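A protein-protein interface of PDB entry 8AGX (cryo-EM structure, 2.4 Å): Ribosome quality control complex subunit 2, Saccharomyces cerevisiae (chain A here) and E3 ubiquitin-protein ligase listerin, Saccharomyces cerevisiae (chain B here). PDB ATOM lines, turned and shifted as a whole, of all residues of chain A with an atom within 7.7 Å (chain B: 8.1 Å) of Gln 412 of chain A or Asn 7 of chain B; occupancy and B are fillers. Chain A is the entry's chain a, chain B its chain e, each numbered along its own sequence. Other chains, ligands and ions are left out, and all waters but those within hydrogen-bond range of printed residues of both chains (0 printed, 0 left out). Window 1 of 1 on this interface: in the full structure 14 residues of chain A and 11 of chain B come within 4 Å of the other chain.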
ATOM      1  N   ALA A 405       3.246  -4.908  -9.905  1.00  0.00           N
ATOM      2  CA  ALA A 405       3.718  -6.209  -9.446  1.00  0.00           C
ATOM      3  C   ALA A 405       2.800  -7.342  -9.900  1.00  0.00           C
ATOM      4  O   ALA A 405       3.269  -8.349 -10.454  1.00  0.00           O
ATOM      5  CB  ALA A 405       3.856  -6.196  -7.928  1.00  0.00           C
ATOM      6  N   VAL A 406       1.489  -7.184  -9.695  1.00  0.00           N
ATOM      7  CA  VAL A 406       0.538  -8.230 -10.072  1.00  0.00           C
ATOM      8  C   VAL A 406       0.492  -8.392 -11.587  1.00  0.00           C
ATOM      9  O   VAL A 406       0.426  -9.513 -12.101  1.00  0.00           O
ATOM     10  CB  VAL A 406      -0.853  -7.932  -9.478  1.00  0.00           C
ATOM     11  CG1 VAL A 406      -1.868  -8.992  -9.882  1.00  0.00           C
ATOM     12  CG2 VAL A 406      -0.775  -7.877  -7.968  1.00  0.00           C
ATOM     13  N   GLN A 407       0.590  -7.285 -12.329  1.00  0.00           N
ATOM     14  CA  GLN A 407       0.608  -7.367 -13.783  1.00  0.00           C
ATOM     15  C   GLN A 407       1.891  -7.997 -14.305  1.00  0.00           C
ATOM     16  O   GLN A 407       1.859  -8.701 -15.320  1.00  0.00           O
ATOM     17  CB  GLN A 407       0.417  -5.977 -14.386  1.00  0.00           C
ATOM     18  CG  GLN A 407       0.047  -5.991 -15.851  1.00  0.00           C
ATOM     19  CD  GLN A 407      -1.422  -6.268 -16.066  1.00  0.00           C
ATOM     20  OE1 GLN A 407      -1.794  -7.268 -16.679  1.00  0.00           O
ATOM     21  NE2 GLN A 407      -2.272  -5.387 -15.558  1.00  0.00           N
ATOM     22  N   GLY A 408       3.021  -7.776 -13.626  1.00  0.00           N
ATOM     23  CA  GLY A 408       4.242  -8.464 -14.007  1.00  0.00           C
ATOM     24  C   GLY A 408       4.166  -9.959 -13.772  1.00  0.00           C
ATOM     25  O   GLY A 408       4.689 -10.746 -14.564  1.00  0.00           O
ATOM     26  N   LEU A 409       3.513 -10.374 -12.685  1.00  0.00           N
ATOM     27  CA  LEU A 409       3.280 -11.806 -12.492  1.00  0.00           C
ATOM     28  C   LEU A 409       2.281 -12.367 -13.501  1.00  0.00           C
ATOM     29  O   LEU A 409       2.387 -13.533 -13.895  1.00  0.00           O
ATOM     30  CB  LEU A 409       2.830 -12.110 -11.062  1.00  0.00           C
ATOM     31  CG  LEU A 409       3.884 -12.284  -9.957  1.00  0.00           C
ATOM     32  CD1 LEU A 409       4.697 -13.503 -10.317  1.00  0.00           C
ATOM     33  CD2 LEU A 409       4.823 -11.122  -9.735  1.00  0.00           C
ATOM     34  N   ILE A 410       1.299 -11.563 -13.913  1.00  0.00           N
ATOM     35  CA  ILE A 410       0.324 -12.012 -14.908  1.00  0.00           C
ATOM     36  C   ILE A 410       0.978 -12.185 -16.273  1.00  0.00           C
ATOM     37  O   ILE A 410       0.735 -13.176 -16.974  1.00  0.00           O
ATOM     38  CB  ILE A 410      -0.870 -11.037 -14.950  1.00  0.00           C
ATOM     39  CG1 ILE A 410      -1.774 -11.265 -13.738  1.00  0.00           C
ATOM     40  CG2 ILE A 410      -1.659 -11.144 -16.245  1.00  0.00           C
ATOM     41  CD1 ILE A 410      -2.973 -10.356 -13.692  1.00  0.00           C
ATOM     42  N   ASP A 411       1.873 -11.267 -16.641  1.00  0.00           N
ATOM     43  CA  ASP A 411       2.507 -11.287 -17.955  1.00  0.00           C
ATOM     44  C   ASP A 411       3.509 -12.419 -18.127  1.00  0.00           C
ATOM     45  O   ASP A 411       3.983 -12.633 -19.247  1.00  0.00           O
ATOM     46  CB  ASP A 411       3.193  -9.952 -18.221  1.00  0.00           C
ATOM     47  CG  ASP A 411       2.206  -8.829 -18.436  1.00  0.00           C
ATOM     48  OD1 ASP A 411       1.005  -9.118 -18.610  1.00  0.00           O
ATOM     49  OD2 ASP A 411       2.629  -7.655 -18.424  1.00  0.00           O
ATOM     50  N   GLN A 412       3.839 -13.148 -17.066  1.00  0.00           N
ATOM     51  CA  GLN A 412       4.628 -14.364 -17.166  1.00  0.00           C
ATOM     52  C   GLN A 412       3.779 -15.580 -17.500  1.00  0.00           C
ATOM     53  O   GLN A 412       4.323 -16.691 -17.542  1.00  0.00           O
ATOM     54  CB  GLN A 412       5.382 -14.612 -15.858  1.00  0.00           C
ATOM     55  CG  GLN A 412       6.316 -13.489 -15.473  1.00  0.00           C
ATOM     56  CD  GLN A 412       7.007 -13.736 -14.152  1.00  0.00           C
ATOM     57  OE1 GLN A 412       7.144 -14.877 -13.714  1.00  0.00           O
ATOM     58  NE2 GLN A 412       7.444 -12.662 -13.506  1.00  0.00           N
ATOM     59  N   GLN A 413       2.473 -15.379 -17.733  1.00  0.00           N
ATOM     60  CA  GLN A 413       1.492 -16.438 -18.002  1.00  0.00           C
ATOM     61  C   GLN A 413       1.469 -17.467 -16.879  1.00  0.00           C
ATOM     62  O   GLN A 413       1.414 -18.674 -17.115  1.00  0.00           O
ATOM     63  CB  GLN A 413       1.734 -17.105 -19.358  1.00  0.00           C
ATOM     64  CG  GLN A 413       1.165 -16.338 -20.527  1.00  0.00           C
ATOM     65  CD  GLN A 413       1.192 -17.147 -21.801  1.00  0.00           C
ATOM     66  OE1 GLN A 413       2.035 -16.929 -22.668  1.00  0.00           O
ATOM     67  NE2 GLN A 413       0.277 -18.100 -21.912  1.00  0.00           N
ATOM     68  N   MET A 414       1.537 -16.980 -15.646  1.00  0.00           N
ATOM     69  CA  MET A 414       1.614 -17.854 -14.493  1.00  0.00           C
ATOM     70  C   MET A 414       0.207 -18.219 -14.036  1.00  0.00           C
ATOM     71  O   MET A 414      -0.739 -17.446 -14.207  1.00  0.00           O
ATOM     72  CB  MET A 414       2.411 -17.162 -13.384  1.00  0.00           C
ATOM     73  CG  MET A 414       2.705 -17.982 -12.139  1.00  0.00           C
ATOM     74  SD  MET A 414       3.658 -17.049 -10.933  1.00  0.00           S
ATOM     75  CE  MET A 414       5.247 -17.000 -11.756  1.00  0.00           C
ATOM     76  N   ASP A 415       0.076 -19.419 -13.475  1.00  0.00           N
ATOM     77  CA  ASP A 415      -1.205 -19.916 -13.001  1.00  0.00           C
ATOM     78  C   ASP A 415      -1.706 -19.076 -11.830  1.00  0.00           C
ATOM     79  O   ASP A 415      -0.931 -18.644 -10.975  1.00  0.00           O
ATOM     80  CB  ASP A 415      -1.074 -21.380 -12.584  1.00  0.00           C
ATOM     81  CG  ASP A 415      -2.400 -22.007 -12.216  1.00  0.00           C
ATOM     82  OD1 ASP A 415      -3.451 -21.491 -12.646  1.00  0.00           O
ATOM     83  OD2 ASP A 415      -2.391 -23.019 -11.488  1.00  0.00           O
ATOM     84  N   ILE A 419      -0.065 -17.929  -8.290  1.00  0.00           N
ATOM     85  CA  ILE A 419       0.123 -16.523  -7.948  1.00  0.00           C
ATOM     86  C   ILE A 419      -0.428 -16.227  -6.557  1.00  0.00           C
ATOM     87  O   ILE A 419       0.227 -15.537  -5.764  1.00  0.00           O
ATOM     88  CB  ILE A 419      -0.514 -15.620  -9.022  1.00  0.00           C
ATOM     89  CG1 ILE A 419       0.296 -15.691 -10.318  1.00  0.00           C
ATOM     90  CG2 ILE A 419      -0.611 -14.175  -8.564  1.00  0.00           C
ATOM     91  CD1 ILE A 419      -0.267 -14.843 -11.441  1.00  0.00           C
ATOM     92  N   LEU A 422       1.966 -17.617  -4.070  1.00  0.00           N
ATOM     93  CA  LEU A 422       3.090 -16.694  -3.984  1.00  0.00           C
ATOM     94  C   LEU A 422       2.758 -15.457  -3.158  1.00  0.00           C
ATOM     95  O   LEU A 422       3.638 -14.937  -2.464  1.00  0.00           O
ATOM     96  CB  LEU A 422       3.527 -16.287  -5.390  1.00  0.00           C
ATOM     97  CG  LEU A 422       4.759 -15.390  -5.509  1.00  0.00           C
ATOM     98  CD1 LEU A 422       5.952 -16.050  -4.862  1.00  0.00           C
ATOM     99  CD2 LEU A 422       5.051 -15.081  -6.955  1.00  0.00           C
ATOM    100  N   SER B   2       9.367 -13.315 -26.391  1.00  0.00           N
ATOM    101  CA  SER B   2       9.948 -14.453 -25.704  1.00  0.00           C
ATOM    102  C   SER B   2       9.421 -14.532 -24.281  1.00  0.00           C
ATOM    103  O   SER B   2       8.275 -14.173 -24.023  1.00  0.00           O
ATOM    104  CB  SER B   2      11.470 -14.343 -25.705  1.00  0.00           C
ATOM    105  OG  SER B   2      12.080 -15.576 -25.364  1.00  0.00           O
ATOM    106  N   PHE B   3      10.253 -14.996 -23.356  1.00  0.00           N
ATOM    107  CA  PHE B   3       9.843 -15.082 -21.960  1.00  0.00           C
ATOM    108  C   PHE B   3       9.599 -13.680 -21.444  1.00  0.00           C
ATOM    109  O   PHE B   3      10.361 -12.766 -21.746  1.00  0.00           O
ATOM    110  CB  PHE B   3      10.919 -15.773 -21.124  1.00  0.00           C
ATOM    111  CG  PHE B   3      11.328 -17.116 -21.650  1.00  0.00           C
ATOM    112  CD1 PHE B   3      10.671 -18.260 -21.242  1.00  0.00           C
ATOM    113  CD2 PHE B   3      12.380 -17.236 -22.544  1.00  0.00           C
ATOM    114  CE1 PHE B   3      11.049 -19.500 -21.719  1.00  0.00           C
ATOM    115  CE2 PHE B   3      12.761 -18.472 -23.027  1.00  0.00           C
ATOM    116  CZ  PHE B   3      12.098 -19.606 -22.610  1.00  0.00           C
ATOM    117  N   GLY B   4       8.549 -13.498 -20.656  1.00  0.00           N
ATOM    118  CA  GLY B   4       8.206 -12.159 -20.201  1.00  0.00           C
ATOM    119  C   GLY B   4       7.866 -12.051 -18.735  1.00  0.00           C
ATOM    120  O   GLY B   4       7.545 -13.055 -18.125  1.00  0.00           O
ATOM    121  N   GLY B   5       7.962 -10.851 -18.166  1.00  0.00           N
ATOM    122  CA  GLY B   5       7.598 -10.631 -16.772  1.00  0.00           C
ATOM    123  C   GLY B   5       8.709 -10.532 -15.746  1.00  0.00           C
ATOM    124  O   GLY B   5       9.807 -11.036 -15.969  1.00  0.00           O
ATOM    125  N   ILE B   6       8.430  -9.883 -14.617  1.00  0.00           N
ATOM    126  CA  ILE B   6       9.436  -9.697 -13.570  1.00  0.00           C
ATOM    127  C   ILE B   6       8.949 -10.284 -12.250  1.00  0.00           C
ATOM    128  O   ILE B   6       7.823 -10.012 -11.831  1.00  0.00           O
ATOM    129  CB  ILE B   6       9.726  -8.200 -13.366  1.00  0.00           C
ATOM    130  CG1 ILE B   6      10.339  -7.595 -14.629  1.00  0.00           C
ATOM    131  CG2 ILE B   6      10.665  -7.972 -12.194  1.00  0.00           C
ATOM    132  CD1 ILE B   6      11.700  -8.159 -14.976  1.00  0.00           C
ATOM    133  N   ASN B   7       9.779 -11.097 -11.597  1.00  0.00           N
ATOM    134  CA  ASN B   7       9.396 -11.708 -10.325  1.00  0.00           C
ATOM    135  C   ASN B   7       9.661 -10.744  -9.194  1.00  0.00           C
ATOM    136  O   ASN B   7      10.599 -10.928  -8.431  1.00  0.00           O
ATOM    137  CB  ASN B   7      10.183 -12.996 -10.091  1.00  0.00           C
ATOM    138  CG  ASN B   7       9.530 -14.203 -10.728  1.00  0.00           C
ATOM    139  OD1 ASN B   7       8.306 -14.313 -10.755  1.00  0.00           O
ATOM    140  ND2 ASN B   7      10.344 -15.125 -11.228  1.00  0.00           N
ATOM    141  N   THR B   8       8.819  -9.731  -9.059  1.00  0.00           N
ATOM    142  CA  THR B   8       9.055  -8.710  -8.055  1.00  0.00           C
ATOM    143  C   THR B   8       9.050  -9.245  -6.644  1.00  0.00           C
ATOM    144  O   THR B   8       9.927  -8.917  -5.854  1.00  0.00           O
ATOM    145  CB  THR B   8       7.941  -7.660  -8.132  1.00  0.00           C
ATOM    146  OG1 THR B   8       6.674  -8.323  -8.087  1.00  0.00           O
ATOM    147  CG2 THR B   8       8.040  -6.879  -9.429  1.00  0.00           C
ATOM    148  N   PHE B   9       8.085 -10.093  -6.327  1.00  0.00           N
ATOM    149  CA  PHE B   9       7.971 -10.596  -4.967  1.00  0.00           C
ATOM    150  C   PHE B   9       9.169 -11.431  -4.587  1.00  0.00           C
ATOM    151  O   PHE B   9       9.686 -11.315  -3.478  1.00  0.00           O
ATOM    152  CB  PHE B   9       6.662 -11.360  -4.799  1.00  0.00           C
ATOM    153  CG  PHE B   9       5.453 -10.485  -4.940  1.00  0.00           C
ATOM    154  CD1 PHE B   9       5.052  -9.668  -3.899  1.00  0.00           C
ATOM    155  CD2 PHE B   9       4.740 -10.451  -6.125  1.00  0.00           C
ATOM    156  CE1 PHE B   9       3.951  -8.850  -4.030  1.00  0.00           C
ATOM    157  CE2 PHE B   9       3.638  -9.632  -6.266  1.00  0.00           C
ATOM    158  CZ  PHE B   9       3.242  -8.829  -5.217  1.00  0.00           C
ATOM    159  N   GLN B  10       9.625 -12.261  -5.511  1.00  0.00           N
ATOM    160  CA  GLN B  10      10.806 -13.062  -5.256  1.00  0.00           C
ATOM    161  C   GLN B  10      12.027 -12.174  -5.070  1.00  0.00           C
ATOM    162  O   GLN B  10      12.862 -12.424  -4.197  1.00  0.00           O
ATOM    163  CB  GLN B  10      11.038 -14.014  -6.424  1.00  0.00           C
ATOM    164  CG  GLN B  10       9.912 -15.003  -6.671  1.00  0.00           C
ATOM    165  CD  GLN B  10      10.090 -16.306  -5.911  1.00  0.00           C
ATOM    166  OE1 GLN B  10      10.803 -16.365  -4.909  1.00  0.00           O
ATOM    167  NE2 GLN B  10       9.439 -17.360  -6.389  1.00  0.00           N
ATOM    168  N   GLN B  11      12.141 -11.140  -5.894  1.00  0.00           N
ATOM    169  CA  GLN B  11      13.297 -10.255  -5.817  1.00  0.00           C
ATOM    170  C   GLN B  11      13.383  -9.518  -4.494  1.00  0.00           C
ATOM    171  O   GLN B  11      14.469  -9.360  -3.945  1.00  0.00           O
ATOM    172  CB  GLN B  11      13.296  -9.275  -6.983  1.00  0.00           C
ATOM    173  CG  GLN B  11      13.687  -9.914  -8.304  1.00  0.00           C
ATOM    174  CD  GLN B  11      13.095  -9.188  -9.490  1.00  0.00           C
ATOM    175  OE1 GLN B  11      12.498  -8.122  -9.345  1.00  0.00           O
ATOM    176  NE2 GLN B  11      13.251  -9.768 -10.675  1.00  0.00           N
ATOM    177  N   TYR B  12      12.250  -9.059  -3.978  1.00  0.00           N
ATOM    178  CA  TYR B  12      12.240  -8.406  -2.673  1.00  0.00           C
ATOM    179  C   TYR B  12      12.654  -9.390  -1.587  1.00  0.00           C
ATOM    180  O   TYR B  12      13.329  -9.010  -0.631  1.00  0.00           O
ATOM    181  CB  TYR B  12      10.876  -7.798  -2.357  1.00  0.00           C
ATOM    182  CG  TYR B  12      10.363  -6.820  -3.394  1.00  0.00           C
ATOM    183  CD1 TYR B  12      11.224  -5.956  -4.054  1.00  0.00           C
ATOM    184  CD2 TYR B  12       9.009  -6.751  -3.699  1.00  0.00           C
ATOM    185  CE1 TYR B  12      10.755  -5.065  -5.000  1.00  0.00           C
ATOM    186  CE2 TYR B  12       8.530  -5.864  -4.640  1.00  0.00           C
ATOM    187  CZ  TYR B  12       9.407  -5.023  -5.287  1.00  0.00           C
ATOM    188  OH  TYR B  12       8.931  -4.135  -6.224  1.00  0.00           O
ATOM    189  N   ASN B  13      12.255 -10.650  -1.722  1.00  0.00           N
ATOM    190  CA  ASN B  13      12.560 -11.662  -0.709  1.00  0.00           C
ATOM    191  C   ASN B  13      14.056 -11.840  -0.531  1.00  0.00           C
ATOM    192  O   ASN B  13      14.509 -12.093   0.585  1.00  0.00           O
ATOM    193  CB  ASN B  13      11.946 -13.000  -1.111  1.00  0.00           C
ATOM    194  CG  ASN B  13      11.903 -13.992   0.030  1.00  0.00           C
ATOM    195  OD1 ASN B  13      11.929 -13.616   1.201  1.00  0.00           O
ATOM    196  ND2 ASN B  13      11.817 -15.272  -0.307  1.00  0.00           N
ATOM    197  N   THR B  14      14.815 -11.759  -1.622  1.00  0.00           N
ATOM    198  CA  THR B  14      16.280 -11.903  -1.564  1.00  0.00           C
ATOM    199  C   THR B  14      16.710 -13.210  -0.920  1.00  0.00           C
ATOM    200  O   THR B  14      17.656 -13.246  -0.135  1.00  0.00           O
ATOM    201  CB  THR B  14      17.015 -10.708  -0.889  1.00  0.00           C
ATOM    202  OG1 THR B  14      16.726 -10.660   0.515  1.00  0.00           O
ATOM    203  CG2 THR B  14      16.635  -9.389  -1.536  1.00  0.00           C
ATOM    204  N   ARG B  24      17.624 -18.414  -6.405  1.00  0.00           N
ATOM    205  CA  ARG B  24      16.536 -18.912  -5.583  1.00  0.00           C
ATOM    206  C   ARG B  24      16.308 -20.375  -5.864  1.00  0.00           C
ATOM    207  O   ARG B  24      16.218 -20.787  -7.017  1.00  0.00           O
ATOM    208  CB  ARG B  24      15.258 -18.134  -5.915  1.00  0.00           C
ATOM    209  CG  ARG B  24      13.986 -18.678  -5.286  1.00  0.00           C
ATOM    210  CD  ARG B  24      13.687 -18.003  -3.958  1.00  0.00           C
ATOM    211  NE  ARG B  24      12.621 -18.675  -3.226  1.00  0.00           N
ATOM    212  CZ  ARG B  24      12.830 -19.629  -2.325  1.00  0.00           C
ATOM    213  NH1 ARG B  24      14.065 -20.014  -2.047  1.00  0.00           N
ATOM    214  NH2 ARG B  24      11.807 -20.194  -1.699  1.00  0.00           N
ATOM    215  N   PHE B  30       5.476 -24.556  -6.366  1.00  0.00           N
ATOM    216  CA  PHE B  30       5.036 -23.186  -6.671  1.00  0.00           C
ATOM    217  C   PHE B  30       6.114 -22.127  -6.819  1.00  0.00           C
ATOM    218  O   PHE B  30       5.986 -21.229  -7.647  1.00  0.00           O
ATOM    219  CB  PHE B  30       3.898 -22.725  -5.738  1.00  0.00           C
ATOM    220  CG  PHE B  30       4.279 -22.630  -4.288  1.00  0.00           C
ATOM    221  CD1 PHE B  30       4.310 -23.758  -3.486  1.00  0.00           C
ATOM    222  CD2 PHE B  30       4.565 -21.400  -3.716  1.00  0.00           C
ATOM    223  CE1 PHE B  30       4.646 -23.667  -2.150  1.00  0.00           C
ATOM    224  CE2 PHE B  30       4.902 -21.302  -2.383  1.00  0.00           C
ATOM    225  CZ  PHE B  30       4.944 -22.436  -1.598  1.00  0.00           C
ATOM    226  N   GLY B  32      10.481 -20.743  -6.695  1.00  0.00           N
ATOM    227  CA  GLY B  32      11.842 -21.120  -7.045  1.00  0.00           C
ATOM    228  C   GLY B  32      11.990 -21.316  -8.532  1.00  0.00           C
ATOM    229  O   GLY B  32      13.043 -21.740  -9.001  1.00  0.00           O
ATOM    230  N   LEU B  33      10.938 -21.011  -9.279  1.00  0.00           N
ATOM    231  CA  LEU B  33      10.990 -21.118 -10.732  1.00  0.00           C
ATOM    232  C   LEU B  33      11.979 -20.112 -11.284  1.00  0.00           C
ATOM    233  O   LEU B  33      12.099 -19.008 -10.759  1.00  0.00           O
ATOM    234  CB  LEU B  33       9.608 -20.838 -11.311  1.00  0.00           C
ATOM    235  CG  LEU B  33       8.501 -21.789 -10.859  1.00  0.00           C
ATOM    236  CD1 LEU B  33       7.132 -21.173 -11.092  1.00  0.00           C
ATOM    237  CD2 LEU B  33       8.629 -23.122 -11.578  1.00  0.00           C
ATOM    238  N   PRO B  34      12.691 -20.485 -12.354  1.00  0.00           N
ATOM    239  CA  PRO B  34      13.703 -19.587 -12.919  1.00  0.00           C
ATOM    240  C   PRO B  34      13.127 -18.298 -13.484  1.00  0.00           C
ATOM    241  O   PRO B  34      12.016 -18.300 -14.012  1.00  0.00           O
ATOM    242  CB  PRO B  34      14.324 -20.418 -14.039  1.00  0.00           C
ATOM    243  CG  PRO B  34      14.058 -21.833 -13.660  1.00  0.00           C
ATOM    244  CD  PRO B  34      12.725 -21.818 -12.975  1.00  0.00           C
ATOM    245  N   ASP B  35      13.879 -17.210 -13.378  1.00  0.00           N
ATOM    246  CA  ASP B  35      13.424 -15.920 -13.878  1.00  0.00           C
ATOM    247  C   ASP B  35      13.239 -15.907 -15.381  1.00  0.00           C
ATOM    248  O   ASP B  35      14.009 -16.524 -16.105  1.00  0.00           O
ATOM    249  CB  ASP B  35      14.441 -14.846 -13.510  1.00  0.00           C
ATOM    250  CG  ASP B  35      13.789 -13.584 -12.981  1.00  0.00           C
ATOM    251  OD1 ASP B  35      12.738 -13.692 -12.316  1.00  0.00           O
ATOM    252  OD2 ASP B  35      14.331 -12.486 -13.221  1.00  0.00           O
ATOM    253  N   PRO B  36      12.225 -15.177 -15.859  1.00  0.00           N
ATOM    254  CA  PRO B  36      12.001 -15.066 -17.301  1.00  0.00           C
ATOM    255  C   PRO B  36      13.191 -14.433 -17.967  1.00  0.00           C
ATOM    256  O   PRO B  36      13.566 -14.829 -19.064  1.00  0.00           O
ATOM    257  CB  PRO B  36      10.818 -14.118 -17.388  1.00  0.00           C
ATOM    258  CG  PRO B  36      10.051 -14.406 -16.150  1.00  0.00           C
ATOM    259  CD  PRO B  36      11.082 -14.656 -15.091  1.00  0.00           C
ATOM    260  N   SER B  37      13.784 -13.451 -17.308  1.00  0.00           N
ATOM    261  CA  SER B  37      14.947 -12.792 -17.867  1.00  0.00           C
ATOM    262  C   SER B  37      16.087 -13.779 -18.057  1.00  0.00           C
ATOM    263  O   SER B  37      16.778 -13.733 -19.062  1.00  0.00           O
ATOM    264  CB  SER B  37      15.398 -11.665 -16.948  1.00  0.00           C
ATOM    265  OG  SER B  37      15.766 -12.164 -15.676  1.00  0.00           O
ATOM    266  N   LEU B  39      15.829 -16.930 -18.593  1.00  0.00           N
ATOM    267  CA  LEU B  39      15.473 -17.742 -19.742  1.00  0.00           C
ATOM    268  C   LEU B  39      15.705 -16.983 -21.046  1.00  0.00           C
ATOM    269  O   LEU B  39      16.157 -17.558 -22.029  1.00  0.00           O
ATOM    270  CB  LEU B  39      14.039 -18.225 -19.595  1.00  0.00           C
ATOM    271  CG  LEU B  39      13.805 -19.029 -18.314  1.00  0.00           C
ATOM    272  CD1 LEU B  39      12.328 -19.205 -18.006  1.00  0.00           C
ATOM    273  CD2 LEU B  39      14.520 -20.369 -18.364  1.00  0.00           C
ATOM    274  N   LEU B  55       9.614 -27.126 -18.062  1.00  0.00           N
ATOM    275  CA  LEU B  55       8.623 -26.419 -17.276  1.00  0.00           C
ATOM    276  C   LEU B  55       7.270 -27.078 -17.426  1.00  0.00           C
ATOM    277  O   LEU B  55       6.502 -27.133 -16.466  1.00  0.00           O
ATOM    278  CB  LEU B  55       8.543 -24.956 -17.699  1.00  0.00           C
ATOM    279  CG  LEU B  55       9.775 -24.110 -17.388  1.00  0.00           C
ATOM    280  CD1 LEU B  55       9.642 -22.719 -17.986  1.00  0.00           C
ATOM    281  CD2 LEU B  55      10.026 -24.045 -15.889  1.00  0.00           C
ATOM    282  N   GLN B  93      18.158 -24.329 -10.826  1.00  0.00           N
ATOM    283  CA  GLN B  93      16.816 -24.068 -10.339  1.00  0.00           C
ATOM    284  C   GLN B  93      15.848 -25.149 -10.781  1.00  0.00           C
ATOM    285  O   GLN B  93      15.045 -25.629  -9.981  1.00  0.00           O
ATOM    286  CB  GLN B  93      16.337 -22.697 -10.804  1.00  0.00           C
ATOM    287  CG  GLN B  93      17.197 -21.554 -10.302  1.00  0.00           C
ATOM    288  CD  GLN B  93      16.488 -20.219 -10.367  1.00  0.00           C
ATOM    289  OE1 GLN B  93      17.048 -19.228 -10.834  1.00  0.00           O
ATOM    290  NE2 GLN B  93      15.249 -20.186  -9.901  1.00  0.00           N
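CB of Ala 405 of chain A touches OG1 of Thr 8 of chain B, 3.5 Å away. O of Gly 408 of chain A touches CA of Gly 5 of chain B, at 3.7 Å. Ile 6 of chain B touches Gly 408 of chain A (N to O, 3.8 Å). Leu 409 of chain A touches Ile 6 of chain B. CD2 of Leu 409 of chain A touches OG1 of Thr 8 of chain B, at 3.7 Å. Leu 409 of chain A touches Phe 9 of chain B (CD2 to CD2, 3.7 Å). O of Asp 411 of chain A touches O of Gly 4 of chain B, at 3.8 Å. Gln 412 of chain A touches Gly 4 of chain B. NE2 of Gln 412 of chain A touches C of Gly 5 of chain B, at 3.3 Å. CD of Gln 412 of chain A touches CG of Pro 36 of chain B (3.7 Å).
The side-chain carboxylate of Asp 35 of chain B lies within hydrogen-bond range of the side-chain amide nitrogen of Asn 7 of chain B (3.0 Å).
Asn 7 of chain B touches two residues of chain A. Printed residues of chain B within 4 Å of Gly 408 of chain A: Gly 5 and Ile 6. Of the printed residues of chain A, Gly 5 of chain B touches Gly 408 and Gln 412. Printed residues of chain A within 4 Å of Phe 9 of chain B: Ala 405 (3.8 Å) and Leu 409 (3.7 Å). Of the printed residues of chain B, Leu 409 of chain A touches Ile 6 (3.8 Å), Asn 7 (3.7 Å), Thr 8 (3.7 Å) and Phe 9 (3.7 Å). Asp 415 of chain A touches none of the printed residues of chain B. The nearest residue of chain A that does not touch Asn 7 of chain B is Met 414 of chain A (4.2 Å). The nearest printed residue of chain B that does not touch Leu 409 of chain A is Gly 5 of chain B (5.8 Å).
The side-chain amide oxygen (OE1) of Gln 412 of chain A lies close to the side-chain amide oxygen (OD1) of Asn 7 of chain B (3.2 Å). N of Ile 6 of chain B lies close to NE2 of Gln 412 of chain A, at 3.2 Å.
Hydrophobic or aromatic side chains of chain B within 4 Å of the printed part of chain A: Phe 9 and Pro 36. Among the printed residues, no Asp or Glu carboxylate lies within 4 Å of a Lys or Arg side-chain nitrogen of the other chain.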
